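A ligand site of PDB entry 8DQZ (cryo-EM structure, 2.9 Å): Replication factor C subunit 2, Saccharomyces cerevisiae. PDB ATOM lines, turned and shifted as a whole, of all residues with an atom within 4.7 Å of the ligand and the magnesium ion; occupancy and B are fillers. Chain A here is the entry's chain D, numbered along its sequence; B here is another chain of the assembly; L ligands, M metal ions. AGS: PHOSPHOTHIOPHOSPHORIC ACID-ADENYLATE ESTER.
O2G of the ligand is bound to the magnesium ion (2.2 Å). The magnesium ion is bound by O2B of the ligand. The magnesium ion has two donor atoms within binding distance. Slightly farther from the magnesium ion lies OG1 of Thr 72 (2.6 Å).
The guanidinium group (NH2) of Arg 155 of chain B lies within hydrogen-bond range of the side-chain amide oxygen (OD1) of Asn 171. The guanidinium group of Arg 184 of chain B is in hydrogen-bond range of the backbone carbonyl oxygen of Arg 155 of chain B, 3.1 Å away. The side-chain carboxylate of Glu 141 is in salt-bridge range of the guanidinium group of Arg 155 of chain B (3.98 Å). The side-chain amino group (NZ) of Lys 71 sits at hydrogen-bond distance from the backbone carbonyl oxygen (O) of Pro 66 (3.0 Å). The side-chain hydroxyl (OG) of Ser 73 sits at hydrogen-bond distance from the guanidinium group (NH1) of Arg 32 (2.7 Å). The backbone carbonyl oxygen of Thr 69 lies within hydrogen-bond range of the side-chain amide nitrogen of Gln 42, at 3.1 Å. The guanidinium group of Arg 184 of chain B is in salt-bridge range of the side-chain carboxylate of Glu 159 of chain B (2.6 Å). NH1 of Arg 184 of chain B lies within hydrogen-bond range of O of Pro 180 of chain B (3.0 Å).
Residues that only touch the magnesium ion: Arg 184 of chain B. The nearest printed residue that does not touch the magnesium ion is Asp 140 (4.1 Å).
NH2 of Arg 229 is in salt-bridge range of O2A of the ligand (2.5 Å). The side-chain hydroxyl of Thr 72 sits close to an oxygen (O2B) of the ligand, at 3.4 Å. O3' of the ligand sits at hydrogen-bond distance from O of Val 28 (2.7 Å). The side-chain amide nitrogen (ND2) of Asn 171 is in hydrogen-bond range of an oxygen (O3G) of the ligand (2.7 Å). S1G of the ligand lies close to NH2 of Arg 155 of chain B, at 3.3 Å. O1B of the ligand lies within hydrogen-bond range of N of Lys 71 (3.1 Å). NZ of Lys 71 is in salt-bridge range of O1B of the ligand (2.8 Å). N of Gly 68 lies within hydrogen-bond range of O3B of the ligand, 2.9 Å away. N of Ser 73 sits at hydrogen-bond distance from O1A of the ligand (3.2 Å). An oxygen (O1A) of the ligand is in hydrogen-bond range of the side-chain hydroxyl (OG) of Ser 73, 2.9 Å away. N of Gly 70 lies within hydrogen-bond range of N7 of the ligand, at 3.1 Å. A nitrogen (N6) of the ligand lies within hydrogen-bond range of the backbone carbonyl oxygen (O) of Thr 69. NH1 of Arg 184 of chain B lies close to S1G of the ligand, at 3.1 Å. NH1 of Arg 32 lies within salt-bridge range of O1A of the ligand, at 3.5 Å. The backbone carbonyl oxygen (O) of Tyr 31 lies within hydrogen-bond range of an oxygen (O2') of the ligand (3.4 Å).
An oxygen (O2A) of the ligand lies close to the side-chain carboxylate of Glu 159 of chain B (3.4 Å). CG of Pro 33 touches C2 of the ligand (3.8 Å). Val 39 touches the ligand. Thr 40 touches the ligand (CG2 to N1, 3.5 Å). Pro 67 touches the ligand (CA to O3G, 3.5 Å). CD1 of Leu 192 touches N6 of the ligand, 3.7 Å away. Leu 228 touches the ligand (CD2 to N3, 3.5 Å). CD1 of Ile 232 touches O2' of the ligand, 3.6 Å away. Pro 180 of chain B touches the ligand. Hydrophobic or aromatic side chains within 4 Å of the ligand: Pro 33, Val 39, Pro 67, Leu 192, Leu 228, Ile 232 and Pro 180 of chain B. 22 residues have an atom within 4 Å of the ligand: Val 28, Tyr 31, Arg 32, Pro 33, Val 39, Thr 40, Pro 67, Gly 68, Thr 69, Gly 70, Lys 71, Thr 72, Ser 73, Asn 171, Leu 192, Leu 228, Arg 229, Ile 232, Arg 155 of chain B, Glu 159 of chain B, Pro 180 of chain B and Arg 184 of chain B. Along chain A the residues within 4 Å of the ligand span positions 28 to 232.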
ATOM      1  N   VAL A  28      19.111  13.153   0.205  1.00  0.00           N
ATOM      2  CA  VAL A  28      18.757  13.878  -1.017  1.00  0.00           C
ATOM      3  C   VAL A  28      18.080  15.203  -0.676  1.00  0.00           C
ATOM      4  O   VAL A  28      18.399  16.244  -1.262  1.00  0.00           O
ATOM      5  CB  VAL A  28      17.877  13.007  -1.926  1.00  0.00           C
ATOM      6  CG1 VAL A  28      18.660  11.811  -2.445  1.00  0.00           C
ATOM      7  CG2 VAL A  28      16.604  12.553  -1.203  1.00  0.00           C
ATOM      8  N   TYR A  31      20.681  17.590   1.614  1.00  0.00           N
ATOM      9  CA  TYR A  31      21.765  18.270   0.915  1.00  0.00           C
ATOM     10  C   TYR A  31      21.285  18.932  -0.376  1.00  0.00           C
ATOM     11  O   TYR A  31      22.074  19.120  -1.308  1.00  0.00           O
ATOM     12  CB  TYR A  31      22.900  17.283   0.627  1.00  0.00           C
ATOM     13  CG  TYR A  31      23.702  16.930   1.854  1.00  0.00           C
ATOM     14  CD1 TYR A  31      24.521  17.866   2.468  1.00  0.00           C
ATOM     15  CD2 TYR A  31      23.653  15.650   2.401  1.00  0.00           C
ATOM     16  CE1 TYR A  31      25.260  17.546   3.587  1.00  0.00           C
ATOM     17  CE2 TYR A  31      24.392  15.330   3.521  1.00  0.00           C
ATOM     18  CZ  TYR A  31      25.192  16.280   4.112  1.00  0.00           C
ATOM     19  OH  TYR A  31      25.931  15.954   5.223  1.00  0.00           O
ATOM     20  N   ARG A  32      20.020  19.294  -0.445  1.00  0.00           N
ATOM     21  CA  ARG A  32      19.523  20.047  -1.593  1.00  0.00           C
ATOM     22  C   ARG A  32      20.184  21.423  -1.612  1.00  0.00           C
ATOM     23  O   ARG A  32      20.249  22.090  -0.564  1.00  0.00           O
ATOM     24  CB  ARG A  32      18.005  20.188  -1.535  1.00  0.00           C
ATOM     25  CG  ARG A  32      17.413  20.975  -2.696  1.00  0.00           C
ATOM     26  CD  ARG A  32      15.897  21.063  -2.589  1.00  0.00           C
ATOM     27  NE  ARG A  32      15.253  19.791  -2.891  1.00  0.00           N
ATOM     28  CZ  ARG A  32      14.895  19.401  -4.106  1.00  0.00           C
ATOM     29  NH1 ARG A  32      15.119  20.148  -5.171  1.00  0.00           N
ATOM     30  NH2 ARG A  32      14.300  18.216  -4.260  1.00  0.00           N
ATOM     31  N   PRO A  33      20.704  21.890  -2.747  1.00  0.00           N
ATOM     32  CA  PRO A  33      21.339  23.208  -2.777  1.00  0.00           C
ATOM     33  C   PRO A  33      20.405  24.291  -2.259  1.00  0.00           C
ATOM     34  O   PRO A  33      19.232  24.360  -2.635  1.00  0.00           O
ATOM     35  CB  PRO A  33      21.673  23.409  -4.257  1.00  0.00           C
ATOM     36  CG  PRO A  33      21.808  22.037  -4.796  1.00  0.00           C
ATOM     37  CD  PRO A  33      20.821  21.197  -4.037  1.00  0.00           C
ATOM     38  N   GLU A  38      25.960  26.578  -4.733  1.00  0.00           N
ATOM     39  CA  GLU A  38      26.063  25.181  -4.344  1.00  0.00           C
ATOM     40  C   GLU A  38      25.729  24.221  -5.481  1.00  0.00           C
ATOM     41  O   GLU A  38      25.767  23.002  -5.284  1.00  0.00           O
ATOM     42  CB  GLU A  38      25.155  24.899  -3.150  1.00  0.00           C
ATOM     43  CG  GLU A  38      25.417  25.789  -1.944  1.00  0.00           C
ATOM     44  CD  GLU A  38      24.708  25.309  -0.697  1.00  0.00           C
ATOM     45  OE1 GLU A  38      25.116  25.719   0.410  1.00  0.00           O
ATOM     46  OE2 GLU A  38      23.743  24.532  -0.819  1.00  0.00           O
ATOM     47  N   VAL A  39      25.398  24.744  -6.664  1.00  0.00           N
ATOM     48  CA  VAL A  39      25.157  23.886  -7.818  1.00  0.00           C
ATOM     49  C   VAL A  39      26.491  23.420  -8.374  1.00  0.00           C
ATOM     50  O   VAL A  39      27.431  24.209  -8.525  1.00  0.00           O
ATOM     51  CB  VAL A  39      24.325  24.616  -8.887  1.00  0.00           C
ATOM     52  CG1 VAL A  39      23.639  23.612  -9.800  1.00  0.00           C
ATOM     53  CG2 VAL A  39      23.283  25.519  -8.229  1.00  0.00           C
ATOM     54  N   THR A  40      26.592  22.121  -8.687  1.00  0.00           N
ATOM     55  CA  THR A  40      27.891  21.519  -8.950  1.00  0.00           C
ATOM     56  C   THR A  40      28.378  21.784 -10.373  1.00  0.00           C
ATOM     57  O   THR A  40      29.442  22.365 -10.573  1.00  0.00           O
ATOM     58  CB  THR A  40      27.840  20.007  -8.657  1.00  0.00           C
ATOM     59  OG1 THR A  40      29.130  19.431  -8.890  1.00  0.00           O
ATOM     60  CG2 THR A  40      26.802  19.291  -9.529  1.00  0.00           C
ATOM     61  N   ALA A  41      27.599  21.367 -11.376  1.00  0.00           N
ATOM     62  CA  ALA A  41      28.077  21.346 -12.754  1.00  0.00           C
ATOM     63  C   ALA A  41      27.023  21.908 -13.706  1.00  0.00           C
ATOM     64  O   ALA A  41      26.686  21.304 -14.730  1.00  0.00           O
ATOM     65  CB  ALA A  41      28.473  19.927 -13.171  1.00  0.00           C
ATOM     66  N   GLN A  42      26.475  23.064 -13.371  1.00  0.00           N
ATOM     67  CA  GLN A  42      25.518  23.772 -14.225  1.00  0.00           C
ATOM     68  C   GLN A  42      25.889  25.252 -14.308  1.00  0.00           C
ATOM     69  O   GLN A  42      25.041  26.143 -14.297  1.00  0.00           O
ATOM     70  CB  GLN A  42      24.100  23.604 -13.706  1.00  0.00           C
ATOM     71  CG  GLN A  42      23.711  22.153 -13.403  1.00  0.00           C
ATOM     72  CD  GLN A  42      23.555  21.322 -14.657  1.00  0.00           C
ATOM     73  OE1 GLN A  42      23.764  21.797 -15.769  1.00  0.00           O
ATOM     74  NE2 GLN A  42      23.179  20.062 -14.479  1.00  0.00           N
ATOM     75  N   PRO A  66      18.110  15.880 -18.332  1.00  0.00           N
ATOM     76  CA  PRO A  66      17.830  14.543 -17.813  1.00  0.00           C
ATOM     77  C   PRO A  66      17.420  14.593 -16.357  1.00  0.00           C
ATOM     78  O   PRO A  66      17.626  15.615 -15.685  1.00  0.00           O
ATOM     79  CB  PRO A  66      19.146  13.789 -18.011  1.00  0.00           C
ATOM     80  CG  PRO A  66      20.202  14.828 -18.228  1.00  0.00           C
ATOM     81  CD  PRO A  66      19.552  16.161 -18.432  1.00  0.00           C
ATOM     82  N   PRO A  67      16.843  13.514 -15.825  1.00  0.00           N
ATOM     83  CA  PRO A  67      16.378  13.549 -14.432  1.00  0.00           C
ATOM     84  C   PRO A  67      17.517  13.756 -13.448  1.00  0.00           C
ATOM     85  O   PRO A  67      18.644  13.313 -13.664  1.00  0.00           O
ATOM     86  CB  PRO A  67      15.723  12.167 -14.242  1.00  0.00           C
ATOM     87  CG  PRO A  67      15.490  11.644 -15.629  1.00  0.00           C
ATOM     88  CD  PRO A  67      16.572  12.224 -16.465  1.00  0.00           C
ATOM     89  N   GLY A  68      17.202  14.434 -12.345  1.00  0.00           N
ATOM     90  CA  GLY A  68      18.143  14.603 -11.257  1.00  0.00           C
ATOM     91  C   GLY A  68      19.389  15.379 -11.619  1.00  0.00           C
ATOM     92  O   GLY A  68      20.500  14.963 -11.266  1.00  0.00           O
ATOM     93  N   THR A  69      19.221  16.509 -12.300  1.00  0.00           N
ATOM     94  CA  THR A  69      20.343  17.356 -12.676  1.00  0.00           C
ATOM     95  C   THR A  69      20.359  18.692 -11.953  1.00  0.00           C
ATOM     96  O   THR A  69      21.366  19.403 -12.038  1.00  0.00           O
ATOM     97  CB  THR A  69      20.342  17.615 -14.191  1.00  0.00           C
ATOM     98  OG1 THR A  69      19.024  18.016 -14.612  1.00  0.00           O
ATOM     99  CG2 THR A  69      20.756  16.360 -14.945  1.00  0.00           C
ATOM    100  N   GLY A  70      19.295  19.058 -11.239  1.00  0.00           N
ATOM    101  CA  GLY A  70      19.297  20.258 -10.439  1.00  0.00           C
ATOM    102  C   GLY A  70      18.491  21.405 -11.028  1.00  0.00           C
ATOM    103  O   GLY A  70      18.903  22.567 -10.924  1.00  0.00           O
ATOM    104  N   LYS A  71      17.349  21.093 -11.631  1.00  0.00           N
ATOM    105  CA  LYS A  71      16.493  22.146 -12.183  1.00  0.00           C
ATOM    106  C   LYS A  71      15.613  22.764 -11.104  1.00  0.00           C
ATOM    107  O   LYS A  71      15.615  23.989 -10.920  1.00  0.00           O
ATOM    108  CB  LYS A  71      15.631  21.570 -13.312  1.00  0.00           C
ATOM    109  CG  LYS A  71      16.424  20.948 -14.451  1.00  0.00           C
ATOM    110  CD  LYS A  71      15.526  20.362 -15.527  1.00  0.00           C
ATOM    111  CE  LYS A  71      14.885  19.050 -15.082  1.00  0.00           C
ATOM    112  NZ  LYS A  71      15.893  17.967 -14.925  1.00  0.00           N
ATOM    113  N   THR A  72      14.868  21.933 -10.381  1.00  0.00           N
ATOM    114  CA  THR A  72      14.009  22.444  -9.314  1.00  0.00           C
ATOM    115  C   THR A  72      14.839  23.146  -8.246  1.00  0.00           C
ATOM    116  O   THR A  72      14.460  24.224  -7.770  1.00  0.00           O
ATOM    117  CB  THR A  72      13.197  21.309  -8.703  1.00  0.00           C
ATOM    118  OG1 THR A  72      12.222  20.850  -9.649  1.00  0.00           O
ATOM    119  CG2 THR A  72      12.487  21.766  -7.440  1.00  0.00           C
ATOM    120  N   SER A  73      15.956  22.541  -7.851  1.00  0.00           N
ATOM    121  CA  SER A  73      16.828  23.172  -6.867  1.00  0.00           C
ATOM    122  C   SER A  73      17.354  24.511  -7.381  1.00  0.00           C
ATOM    123  O   SER A  73      17.408  25.495  -6.639  1.00  0.00           O
ATOM    124  CB  SER A  73      17.990  22.248  -6.524  1.00  0.00           C
ATOM    125  OG  SER A  73      17.515  21.008  -6.014  1.00  0.00           O
ATOM    126  N   ASP A 140       6.371  23.561 -13.087  1.00  0.00           N
ATOM    127  CA  ASP A 140       7.230  22.389 -13.067  1.00  0.00           C
ATOM    128  C   ASP A 140       6.555  21.221 -13.787  1.00  0.00           C
ATOM    129  O   ASP A 140       5.325  21.093 -13.794  1.00  0.00           O
ATOM    130  CB  ASP A 140       7.555  21.991 -11.631  1.00  0.00           C
ATOM    131  CG  ASP A 140       8.937  21.368 -11.505  1.00  0.00           C
ATOM    132  OD1 ASP A 140       9.620  21.629 -10.485  1.00  0.00           O
ATOM    133  OD2 ASP A 140       9.338  20.623 -12.417  1.00  0.00           O
ATOM    134  N   GLU A 141       7.367  20.365 -14.398  1.00  0.00           N
ATOM    135  CA  GLU A 141       6.869  19.229 -15.170  1.00  0.00           C
ATOM    136  C   GLU A 141       5.869  19.688 -16.221  1.00  0.00           C
ATOM    137  O   GLU A 141       4.794  19.114 -16.372  1.00  0.00           O
ATOM    138  CB  GLU A 141       6.256  18.175 -14.247  1.00  0.00           C
ATOM    139  CG  GLU A 141       7.247  17.580 -13.263  1.00  0.00           C
ATOM    140  CD  GLU A 141       6.698  17.509 -11.851  1.00  0.00           C
ATOM    141  OE1 GLU A 141       5.469  17.393 -11.686  1.00  0.00           O
ATOM    142  OE2 GLU A 141       7.507  17.570 -10.910  1.00  0.00           O
ATOM    143  N   ASN A 171      11.535  17.588 -18.652  1.00  0.00           N
ATOM    144  CA  ASN A 171      12.565  16.599 -18.978  1.00  0.00           C
ATOM    145  C   ASN A 171      12.645  16.302 -20.459  1.00  0.00           C
ATOM    146  O   ASN A 171      13.746  16.136 -20.992  1.00  0.00           O
ATOM    147  CB  ASN A 171      12.311  15.299 -18.219  1.00  0.00           C
ATOM    148  CG  ASN A 171      12.784  15.355 -16.779  1.00  0.00           C
ATOM    149  OD1 ASN A 171      11.987  15.312 -15.848  1.00  0.00           O
ATOM    150  ND2 ASN A 171      14.093  15.444 -16.589  1.00  0.00           N
ATOM    151  N   LEU A 192      25.164  14.713 -14.746  1.00  0.00           N
ATOM    152  CA  LEU A 192      26.129  14.774 -13.645  1.00  0.00           C
ATOM    153  C   LEU A 192      26.841  13.429 -13.563  1.00  0.00           C
ATOM    154  O   LEU A 192      26.317  12.476 -12.969  1.00  0.00           O
ATOM    155  CB  LEU A 192      25.422  15.124 -12.348  1.00  0.00           C
ATOM    156  CG  LEU A 192      24.622  16.430 -12.310  1.00  0.00           C
ATOM    157  CD1 LEU A 192      24.446  16.916 -10.885  1.00  0.00           C
ATOM    158  CD2 LEU A 192      25.281  17.508 -13.164  1.00  0.00           C
ATOM    159  N   ARG A 200      30.825  17.180  -5.157  1.00  0.00           N
ATOM    160  CA  ARG A 200      29.661  17.237  -4.277  1.00  0.00           C
ATOM    161  C   ARG A 200      29.474  15.932  -3.513  1.00  0.00           C
ATOM    162  O   ARG A 200      29.175  15.943  -2.316  1.00  0.00           O
ATOM    163  CB  ARG A 200      28.402  17.559  -5.099  1.00  0.00           C
ATOM    164  CG  ARG A 200      27.139  17.751  -4.276  1.00  0.00           C
ATOM    165  CD  ARG A 200      27.228  18.995  -3.394  1.00  0.00           C
ATOM    166  NE  ARG A 200      25.974  19.254  -2.698  1.00  0.00           N
ATOM    167  CZ  ARG A 200      25.788  20.261  -1.847  1.00  0.00           C
ATOM    168  NH1 ARG A 200      26.756  21.116  -1.560  1.00  0.00           N
ATOM    169  NH2 ARG A 200      24.594  20.407  -1.279  1.00  0.00           N
ATOM    170  N   LEU A 228      22.514  12.462  -9.928  1.00  0.00           N
ATOM    171  CA  LEU A 228      23.194  12.625  -8.650  1.00  0.00           C
ATOM    172  C   LEU A 228      22.297  12.205  -7.483  1.00  0.00           C
ATOM    173  O   LEU A 228      22.798  11.811  -6.428  1.00  0.00           O
ATOM    174  CB  LEU A 228      23.657  14.072  -8.481  1.00  0.00           C
ATOM    175  CG  LEU A 228      24.552  14.357  -7.266  1.00  0.00           C
ATOM    176  CD1 LEU A 228      25.749  13.422  -7.227  1.00  0.00           C
ATOM    177  CD2 LEU A 228      25.015  15.811  -7.282  1.00  0.00           C
ATOM    178  N   ARG A 229      20.972  12.312  -7.648  1.00  0.00           N
ATOM    179  CA  ARG A 229      20.071  11.844  -6.606  1.00  0.00           C
ATOM    180  C   ARG A 229      20.242  10.354  -6.370  1.00  0.00           C
ATOM    181  O   ARG A 229      20.273   9.897  -5.214  1.00  0.00           O
ATOM    182  CB  ARG A 229      18.623  12.152  -6.992  1.00  0.00           C
ATOM    183  CG  ARG A 229      17.610  11.871  -5.896  1.00  0.00           C
ATOM    184  CD  ARG A 229      16.182  11.936  -6.421  1.00  0.00           C
ATOM    185  NE  ARG A 229      15.778  13.290  -6.788  1.00  0.00           N
ATOM    186  CZ  ARG A 229      15.447  13.684  -8.018  1.00  0.00           C
ATOM    187  NH1 ARG A 229      15.477  12.846  -9.046  1.00  0.00           N
ATOM    188  NH2 ARG A 229      15.088  14.945  -8.216  1.00  0.00           N
ATOM    189  N   ILE A 232      23.460   9.815  -4.428  1.00  0.00           N
ATOM    190  CA  ILE A 232      23.307  10.147  -3.021  1.00  0.00           C
ATOM    191  C   ILE A 232      22.529   9.050  -2.290  1.00  0.00           C
ATOM    192  O   ILE A 232      22.869   8.667  -1.163  1.00  0.00           O
ATOM    193  CB  ILE A 232      22.632  11.514  -2.852  1.00  0.00           C
ATOM    194  CG1 ILE A 232      23.517  12.622  -3.443  1.00  0.00           C
ATOM    195  CG2 ILE A 232      22.341  11.800  -1.393  1.00  0.00           C
ATOM    196  CD1 ILE A 232      22.772  13.899  -3.757  1.00  0.00           C
ATOM    197  N   ARG B 155       5.575  12.487  -8.335  1.00  0.00           N
ATOM    198  CA  ARG B 155       6.968  12.943  -8.349  1.00  0.00           C
ATOM    199  C   ARG B 155       7.239  13.974  -7.261  1.00  0.00           C
ATOM    200  O   ARG B 155       8.049  13.729  -6.358  1.00  0.00           O
ATOM    201  CB  ARG B 155       7.308  13.530  -9.725  1.00  0.00           C
ATOM    202  CG  ARG B 155       7.525  12.490 -10.807  1.00  0.00           C
ATOM    203  CD  ARG B 155       7.791  13.132 -12.161  1.00  0.00           C
ATOM    204  NE  ARG B 155       8.920  14.052 -12.129  1.00  0.00           N
ATOM    205  CZ  ARG B 155       9.363  14.730 -13.179  1.00  0.00           C
ATOM    206  NH1 ARG B 155       8.801  14.611 -14.363  1.00  0.00           N
ATOM    207  NH2 ARG B 155      10.405  15.540 -13.028  1.00  0.00           N
ATOM    208  N   ARG B 156       6.570  15.127  -7.311  1.00  0.00           N
ATOM    209  CA  ARG B 156       6.846  16.200  -6.371  1.00  0.00           C
ATOM    210  C   ARG B 156       6.187  15.997  -5.006  1.00  0.00           C
ATOM    211  O   ARG B 156       6.675  16.551  -4.016  1.00  0.00           O
ATOM    212  CB  ARG B 156       6.392  17.545  -6.939  1.00  0.00           C
ATOM    213  CG  ARG B 156       7.336  18.128  -7.972  1.00  0.00           C
ATOM    214  CD  ARG B 156       8.638  18.624  -7.355  1.00  0.00           C
ATOM    215  NE  ARG B 156       8.477  19.890  -6.662  1.00  0.00           N
ATOM    216  CZ  ARG B 156       9.288  20.334  -5.711  1.00  0.00           C
ATOM    217  NH1 ARG B 156      10.335  19.625  -5.298  1.00  0.00           N
ATOM    218  NH2 ARG B 156       9.044  21.512  -5.142  1.00  0.00           N
ATOM    219  N   GLU B 159       8.709  14.536  -2.795  1.00  0.00           N
ATOM    220  CA  GLU B 159       9.794  15.414  -2.377  1.00  0.00           C
ATOM    221  C   GLU B 159       9.356  16.490  -1.386  1.00  0.00           C
ATOM    222  O   GLU B 159      10.035  16.692  -0.374  1.00  0.00           O
ATOM    223  CB  GLU B 159      10.416  16.093  -3.591  1.00  0.00           C
ATOM    224  CG  GLU B 159      11.198  15.153  -4.495  1.00  0.00           C
ATOM    225  CD  GLU B 159      12.023  15.889  -5.538  1.00  0.00           C
ATOM    226  OE1 GLU B 159      13.144  16.336  -5.205  1.00  0.00           O
ATOM    227  OE2 GLU B 159      11.548  16.039  -6.681  1.00  0.00           O
ATOM    228  N   PRO B 180      11.882   9.314 -13.675  1.00  0.00           N
ATOM    229  CA  PRO B 180      11.853  10.296 -12.575  1.00  0.00           C
ATOM    230  C   PRO B 180      11.422   9.705 -11.246  1.00  0.00           C
ATOM    231  O   PRO B 180      11.996  10.044 -10.208  1.00  0.00           O
ATOM    232  CB  PRO B 180      10.849  11.347 -13.082  1.00  0.00           C
ATOM    233  CG  PRO B 180      10.920  11.236 -14.567  1.00  0.00           C
ATOM    234  CD  PRO B 180      11.135   9.788 -14.849  1.00  0.00           C
ATOM    235  N   ARG B 184      13.699   8.627  -7.436  1.00  0.00           N
ATOM    236  CA  ARG B 184      13.314   9.147  -6.135  1.00  0.00           C
ATOM    237  C   ARG B 184      13.152   8.054  -5.079  1.00  0.00           C
ATOM    238  O   ARG B 184      12.760   8.374  -3.945  1.00  0.00           O
ATOM    239  CB  ARG B 184      12.009   9.933  -6.246  1.00  0.00           C
ATOM    240  CG  ARG B 184      12.108  11.205  -7.075  1.00  0.00           C
ATOM    241  CD  ARG B 184      10.737  11.824  -7.305  1.00  0.00           C
ATOM    242  NE  ARG B 184      10.819  13.243  -7.619  1.00  0.00           N
ATOM    243  CZ  ARG B 184      11.073  13.736  -8.827  1.00  0.00           C
ATOM    244  NH1 ARG B 184      11.281  12.946  -9.858  1.00  0.00           N
ATOM    245  NH2 ARG B 184      11.111  15.058  -8.995  1.00  0.00           N
HETATM  246  PG  AGS L   1      13.701  15.836 -12.335  1.00  0.00           P
HETATM  247  S1G AGS L   1      13.146  14.003 -12.142  1.00  0.00           S
HETATM  248  O2G AGS L   1      12.486  16.839 -11.807  1.00  0.00           O
HETATM  249  O3G AGS L   1      14.048  16.151 -13.950  1.00  0.00           O
HETATM  250  PB  AGS L   1      15.589  17.568 -10.949  1.00  0.00           P
HETATM  251  O1B AGS L   1      16.189  18.289 -12.143  1.00  0.00           O
HETATM  252  O2B AGS L   1      14.437  18.383 -10.403  1.00  0.00           O
HETATM  253  O3B AGS L   1      15.044  16.081 -11.405  1.00  0.00           O
HETATM  254  PA  AGS L   1      16.528  17.917  -8.276  1.00  0.00           P
HETATM  255  O1A AGS L   1      16.548  19.418  -8.274  1.00  0.00           O
HETATM  256  O2A AGS L   1      15.199  17.430  -7.735  1.00  0.00           O
HETATM  257  O3A AGS L   1      16.725  17.385  -9.790  1.00  0.00           O
HETATM  258  O5' AGS L   1      17.769  17.338  -7.307  1.00  0.00           O
HETATM  259  C5' AGS L   1      17.452  16.371  -6.363  1.00  0.00           C
HETATM  260  C4' AGS L   1      18.645  16.116  -5.491  1.00  0.00           C
HETATM  261  O4' AGS L   1      19.635  15.647  -6.210  1.00  0.00           O
HETATM  262  C3' AGS L   1      19.149  17.558  -4.825  1.00  0.00           C
HETATM  263  O3' AGS L   1      18.532  17.742  -3.487  1.00  0.00           O
HETATM  264  C2' AGS L   1      20.376  17.470  -4.723  1.00  0.00           C
HETATM  265  O2' AGS L   1      20.735  16.826  -3.434  1.00  0.00           O
HETATM  266  C1' AGS L   1      20.823  16.541  -5.955  1.00  0.00           C
HETATM  267  N9  AGS L   1      21.082  17.243  -7.049  1.00  0.00           N
HETATM  268  C8  AGS L   1      20.528  17.285  -8.256  1.00  0.00           C
HETATM  269  N7  AGS L   1      21.202  18.173  -8.995  1.00  0.00           N
HETATM  270  C5  AGS L   1      22.184  18.676  -8.235  1.00  0.00           C
HETATM  271  C6  AGS L   1      23.155  19.611  -8.493  1.00  0.00           C
HETATM  272  N6  AGS L   1      23.365  20.321  -9.762  1.00  0.00           N
HETATM  273  N1  AGS L   1      24.019  19.936  -7.558  1.00  0.00           N
HETATM  274  C2  AGS L   1      23.952  19.351  -6.344  1.00  0.00           C
HETATM  275  N3  AGS L   1      22.996  18.437  -6.099  1.00  0.00           N
HETATM  276  C4  AGS L   1      22.120  18.104  -7.041  1.00  0.00           C
HETATM  277 MG    MG M   1      11.986  18.294 -10.276  1.00  0.00          MG
